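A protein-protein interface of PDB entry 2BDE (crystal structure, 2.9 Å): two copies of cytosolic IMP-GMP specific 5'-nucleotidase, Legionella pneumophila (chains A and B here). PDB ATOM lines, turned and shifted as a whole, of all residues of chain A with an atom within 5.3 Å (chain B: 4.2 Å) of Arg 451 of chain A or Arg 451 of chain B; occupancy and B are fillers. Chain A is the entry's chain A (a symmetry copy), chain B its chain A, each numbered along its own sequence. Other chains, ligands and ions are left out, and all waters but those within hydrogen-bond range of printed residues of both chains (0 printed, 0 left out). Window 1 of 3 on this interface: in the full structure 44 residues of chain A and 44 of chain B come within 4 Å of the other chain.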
ATOM      1  N   ARG A  86      -5.319  35.795 -27.448  1.00  0.00           N
ATOM      2  CA  ARG A  86      -3.923  35.911 -27.058  1.00  0.00           C
ATOM      3  C   ARG A  86      -3.180  36.935 -27.904  1.00  0.00           C
ATOM      4  O   ARG A  86      -2.207  37.521 -27.453  1.00  0.00           O
ATOM      5  CB  ARG A  86      -3.251  34.538 -27.180  1.00  0.00           C
ATOM      6  CG  ARG A  86      -1.725  34.535 -27.227  1.00  0.00           C
ATOM      7  CD  ARG A  86      -1.192  33.112 -27.473  1.00  0.00           C
ATOM      8  NE  ARG A  86      -1.953  32.424 -28.525  1.00  0.00           N
ATOM      9  CZ  ARG A  86      -1.586  31.290 -29.117  1.00  0.00           C
ATOM     10  NH1 ARG A  86      -0.452  30.693 -28.769  1.00  0.00           N
ATOM     11  NH2 ARG A  86      -2.355  30.761 -30.061  1.00  0.00           N
ATOM     12  N   ARG A 411      -9.872  31.222 -21.942  1.00  0.00           N
ATOM     13  CA  ARG A 411     -10.067  30.870 -23.348  1.00  0.00           C
ATOM     14  C   ARG A 411     -10.752  31.947 -24.184  1.00  0.00           C
ATOM     15  O   ARG A 411     -11.701  32.591 -23.738  1.00  0.00           O
ATOM     16  CB  ARG A 411     -10.883  29.578 -23.461  1.00  0.00           C
ATOM     17  CG  ARG A 411     -10.164  28.332 -22.977  1.00  0.00           C
ATOM     18  CD  ARG A 411      -9.081  27.921 -23.953  1.00  0.00           C
ATOM     19  NE  ARG A 411      -8.280  26.811 -23.454  1.00  0.00           N
ATOM     20  CZ  ARG A 411      -7.320  26.211 -24.154  1.00  0.00           C
ATOM     21  NH1 ARG A 411      -7.046  26.616 -25.389  1.00  0.00           N
ATOM     22  NH2 ARG A 411      -6.627  25.212 -23.618  1.00  0.00           N
ATOM     23  N   GLU A 416      -6.029  30.438 -26.322  1.00  0.00           N
ATOM     24  CA  GLU A 416      -6.074  31.114 -25.048  1.00  0.00           C
ATOM     25  C   GLU A 416      -6.488  32.576 -25.194  1.00  0.00           C
ATOM     26  O   GLU A 416      -6.345  33.175 -26.257  1.00  0.00           O
ATOM     27  CB  GLU A 416      -4.721  31.016 -24.341  1.00  0.00           C
ATOM     28  CG  GLU A 416      -3.507  31.235 -25.221  1.00  0.00           C
ATOM     29  CD  GLU A 416      -3.029  29.955 -25.883  1.00  0.00           C
ATOM     30  OE1 GLU A 416      -3.691  29.482 -26.840  1.00  0.00           O
ATOM     31  OE2 GLU A 416      -1.984  29.420 -25.437  1.00  0.00           O
ATOM     32  N   ASP A 424       0.650  33.852 -18.327  1.00  0.00           N
ATOM     33  CA  ASP A 424       1.777  33.088 -18.843  1.00  0.00           C
ATOM     34  C   ASP A 424       3.070  33.901 -18.868  1.00  0.00           C
ATOM     35  O   ASP A 424       4.142  33.403 -18.511  1.00  0.00           O
ATOM     36  CB  ASP A 424       1.474  32.610 -20.259  1.00  0.00           C
ATOM     37  CG  ASP A 424       2.585  31.750 -20.833  1.00  0.00           C
ATOM     38  OD1 ASP A 424       2.839  31.835 -22.054  1.00  0.00           O
ATOM     39  OD2 ASP A 424       3.198  30.983 -20.066  1.00  0.00           O
ATOM     40  N   ASN A 449       5.889  21.821 -17.723  1.00  0.00           N
ATOM     41  CA  ASN A 449       5.699  20.777 -18.715  1.00  0.00           C
ATOM     42  C   ASN A 449       6.138  21.340 -20.046  1.00  0.00           C
ATOM     43  O   ASN A 449       5.891  22.509 -20.322  1.00  0.00           O
ATOM     44  CB  ASN A 449       4.231  20.400 -18.809  1.00  0.00           C
ATOM     45  CG  ASN A 449       3.624  20.141 -17.461  1.00  0.00           C
ATOM     46  OD1 ASN A 449       4.079  19.268 -16.723  1.00  0.00           O
ATOM     47  ND2 ASN A 449       2.593  20.906 -17.118  1.00  0.00           N
ATOM     48  N   ARG A 450       6.785  20.524 -20.875  1.00  0.00           N
ATOM     49  CA  ARG A 450       7.231  21.006 -22.177  1.00  0.00           C
ATOM     50  C   ARG A 450       6.032  21.402 -23.022  1.00  0.00           C
ATOM     51  O   ARG A 450       4.992  20.744 -23.008  1.00  0.00           O
ATOM     52  CB  ARG A 450       8.061  19.941 -22.903  1.00  0.00           C
ATOM     53  CG  ARG A 450       9.572  20.045 -22.647  1.00  0.00           C
ATOM     54  CD  ARG A 450      10.356  20.701 -23.810  1.00  0.00           C
ATOM     55  NE  ARG A 450      10.453  19.836 -24.992  1.00  0.00           N
ATOM     56  CZ  ARG A 450      11.211  20.091 -26.062  1.00  0.00           C
ATOM     57  NH1 ARG A 450      11.954  21.194 -26.112  1.00  0.00           N
ATOM     58  NH2 ARG A 450      11.228  19.244 -27.090  1.00  0.00           N
ATOM     59  N   ARG A 451       6.190  22.491 -23.760  1.00  0.00           N
ATOM     60  CA  ARG A 451       5.121  22.991 -24.594  1.00  0.00           C
ATOM     61  C   ARG A 451       4.795  22.030 -25.729  1.00  0.00           C
ATOM     62  O   ARG A 451       3.690  21.491 -25.777  1.00  0.00           O
ATOM     63  CB  ARG A 451       5.488  24.373 -25.146  1.00  0.00           C
ATOM     64  CG  ARG A 451       4.281  25.273 -25.452  1.00  0.00           C
ATOM     65  CD  ARG A 451       3.468  24.774 -26.662  1.00  0.00           C
ATOM     66  NE  ARG A 451       2.409  25.707 -27.052  1.00  0.00           N
ATOM     67  CZ  ARG A 451       1.811  25.709 -28.243  1.00  0.00           C
ATOM     68  NH1 ARG A 451       2.167  24.823 -29.172  1.00  0.00           N
ATOM     69  NH2 ARG A 451       0.861  26.603 -28.509  1.00  0.00           N
ATOM     70  N   LEU A 452       5.758  21.811 -26.624  1.00  0.00           N
ATOM     71  CA  LEU A 452       5.599  20.926 -27.789  1.00  0.00           C
ATOM     72  C   LEU A 452       4.953  21.681 -28.960  1.00  0.00           C
ATOM     73  O   LEU A 452       3.764  22.016 -28.932  1.00  0.00           O
ATOM     74  CB  LEU A 452       4.758  19.686 -27.447  1.00  0.00           C
ATOM     75  CG  LEU A 452       5.101  18.405 -28.219  1.00  0.00           C
ATOM     76  CD1 LEU A 452       5.963  17.502 -27.345  1.00  0.00           C
ATOM     77  CD2 LEU A 452       3.838  17.677 -28.617  1.00  0.00           C
ATOM     78  N   LEU A 453       5.750  21.938 -29.991  1.00  0.00           N
ATOM     79  CA  LEU A 453       5.293  22.672 -31.166  1.00  0.00           C
ATOM     80  C   LEU A 453       4.620  21.781 -32.192  1.00  0.00           C
ATOM     81  O   LEU A 453       4.815  20.571 -32.199  1.00  0.00           O
ATOM     82  CB  LEU A 453       6.481  23.383 -31.803  1.00  0.00           C
ATOM     83  CG  LEU A 453       7.225  24.272 -30.809  1.00  0.00           C
ATOM     84  CD1 LEU A 453       8.496  24.777 -31.438  1.00  0.00           C
ATOM     85  CD2 LEU A 453       6.331  25.428 -30.380  1.00  0.00           C
ATOM     86  N   ALA A 454       3.832  22.387 -33.068  1.00  0.00           N
ATOM     87  CA  ALA A 454       3.122  21.631 -34.087  1.00  0.00           C
ATOM     88  C   ALA A 454       4.037  20.679 -34.845  1.00  0.00           C
ATOM     89  O   ALA A 454       3.674  19.535 -35.083  1.00  0.00           O
ATOM     90  CB  ALA A 454       2.433  22.579 -35.057  1.00  0.00           C
ATOM     91  N   GLU B 416       9.700  28.101 -26.449  1.00  0.00           N
ATOM     92  CA  GLU B 416       9.899  28.464 -27.831  1.00  0.00           C
ATOM     93  C   GLU B 416      10.718  29.745 -27.969  1.00  0.00           C
ATOM     94  O   GLU B 416      10.784  30.561 -27.053  1.00  0.00           O
ATOM     95  CB  GLU B 416       8.555  28.619 -28.543  1.00  0.00           C
ATOM     96  CG  GLU B 416       7.481  29.348 -27.762  1.00  0.00           C
ATOM     97  CD  GLU B 416       6.676  28.419 -26.871  1.00  0.00           C
ATOM     98  OE1 GLU B 416       7.204  27.979 -25.819  1.00  0.00           O
ATOM     99  OE2 GLU B 416       5.509  28.127 -27.231  1.00  0.00           O
ATOM    100  N   ASN B 449      -4.435  21.709 -33.489  1.00  0.00           N
ATOM    101  CA  ASN B 449      -4.523  20.876 -32.303  1.00  0.00           C
ATOM    102  C   ASN B 449      -4.743  21.797 -31.126  1.00  0.00           C
ATOM    103  O   ASN B 449      -4.162  22.877 -31.084  1.00  0.00           O
ATOM    104  CB  ASN B 449      -3.222  20.122 -32.091  1.00  0.00           C
ATOM    105  CG  ASN B 449      -2.754  19.434 -33.341  1.00  0.00           C
ATOM    106  OD1 ASN B 449      -3.462  18.599 -33.902  1.00  0.00           O
ATOM    107  ND2 ASN B 449      -1.558  19.787 -33.800  1.00  0.00           N
ATOM    108  N   ARG B 450      -5.570  21.385 -30.170  1.00  0.00           N
ATOM    109  CA  ARG B 450      -5.821  22.226 -29.005  1.00  0.00           C
ATOM    110  C   ARG B 450      -4.534  22.423 -28.221  1.00  0.00           C
ATOM    111  O   ARG B 450      -3.728  21.506 -28.072  1.00  0.00           O
ATOM    112  CB  ARG B 450      -6.899  21.612 -28.105  1.00  0.00           C
ATOM    113  CG  ARG B 450      -8.325  22.090 -28.420  1.00  0.00           C
ATOM    114  CD  ARG B 450      -8.852  23.163 -27.437  1.00  0.00           C
ATOM    115  NE  ARG B 450      -9.159  22.618 -26.109  1.00  0.00           N
ATOM    116  CZ  ARG B 450      -9.779  23.289 -25.135  1.00  0.00           C
ATOM    117  NH1 ARG B 450     -10.173  24.545 -25.330  1.00  0.00           N
ATOM    118  NH2 ARG B 450     -10.007  22.707 -23.959  1.00  0.00           N
ATOM    119  N   ARG B 451      -4.352  23.637 -27.723  1.00  0.00           N
ATOM    120  CA  ARG B 451      -3.160  23.967 -26.975  1.00  0.00           C
ATOM    121  C   ARG B 451      -3.090  23.202 -25.660  1.00  0.00           C
ATOM    122  O   ARG B 451      -2.184  22.391 -25.473  1.00  0.00           O
ATOM    123  CB  ARG B 451      -3.100  25.478 -26.723  1.00  0.00           C
ATOM    124  CG  ARG B 451      -1.678  26.038 -26.569  1.00  0.00           C
ATOM    125  CD  ARG B 451      -1.005  25.581 -25.259  1.00  0.00           C
ATOM    126  NE  ARG B 451       0.287  26.230 -25.033  1.00  0.00           N
ATOM    127  CZ  ARG B 451       0.896  26.301 -23.850  1.00  0.00           C
ATOM    128  NH1 ARG B 451       0.329  25.759 -22.773  1.00  0.00           N
ATOM    129  NH2 ARG B 451       2.070  26.920 -23.741  1.00  0.00           N
ATOM    130  N   LEU B 452      -4.048  23.452 -24.768  1.00  0.00           N
ATOM    131  CA  LEU B 452      -4.114  22.812 -23.445  1.00  0.00           C
ATOM    132  C   LEU B 452      -3.245  23.570 -22.432  1.00  0.00           C
ATOM    133  O   LEU B 452      -2.011  23.538 -22.490  1.00  0.00           O
ATOM    134  CB  LEU B 452      -3.674  21.342 -23.506  1.00  0.00           C
ATOM    135  CG  LEU B 452      -4.346  20.395 -22.503  1.00  0.00           C
ATOM    136  CD1 LEU B 452      -5.456  19.619 -23.203  1.00  0.00           C
ATOM    137  CD2 LEU B 452      -3.333  19.431 -21.929  1.00  0.00           C
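The guanidinium group (NE) of Arg 451 of chain B is in salt-bridge range of the side-chain carboxylate (OE2) of Glu 416 of chain A, 3.9 Å away.
The guanidinium group (NE) of Arg 451 of chain A sits close to the guanidinium group (NE) of Arg 451 of chain B (3.0 Å).
NE of Arg 411 of chain A sits close to NH1 of Arg 450 of chain B.
The guanidinium group of Arg 451 of chain A lies within salt-bridge range of the side-chain carboxylate of Glu 416 of chain B, 3.9 Å away.
NH2 of Arg 411 of chain A sits close to N of Leu 452 of chain B (3.3 Å).
The side-chain carboxylate (OE1) of Glu 416 of chain A lies within salt-bridge range of the guanidinium group (NH2) of Arg 86 of chain A (3.7 Å).
Glu 416 of chain A touches Arg 451 of chain B, and with the chains exchanged Arg 451 of chain A touches Glu 416 of chain B.
Arg 451 of chain A touches its own counterpart, Arg 451 of chain B.
5 positions are printed for both chains.
Printed residues of chain B within 4 Å of Arg 411 of chain A: Arg 450 (3.5 Å) and Leu 452 (3.3 Å).
Of the printed residues of chain B, Glu 416 of chain A touches Arg 451.
Of the printed residues of chain A, Glu 416 of chain B touches Arg 451 (3.6 Å).
Printed residues of chain A within 4 Å of Arg 450 of chain B: Arg 411.
Of chain A, only Glu 416 (3.6 Å) and Arg 451 (3.0 Å) come within 4 Å of Arg 451 of chain B.
Of the printed residues of chain A, Leu 452 of chain B touches Arg 411 (3.3 Å).
The nearest printed residue of chain A that does not touch Arg 450 of chain B is Arg 451 of chain A (6.8 Å).
Of the 5 printed residues of chain B, 4 touch a printed residue of chain A.
Of the 10 printed residues of chain A, 3 touch a printed residue of chain B.
Printed residues of chain A that touch a printed residue of chain B: Arg 411, Glu 416 and Arg 451.
Along chain A the printed residues that touch a printed residue of chain B span positions 411 to 451.
Among the printed residues, 5 pairs touch across the chains.
Among the printed residues, Asp or Glu carboxylates within 4 Å of a Lys or Arg side-chain nitrogen of the other chain: Glu 416 of chain A with Arg 451 of chain B and Arg 451 of chain A with Glu 416 of chain B.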
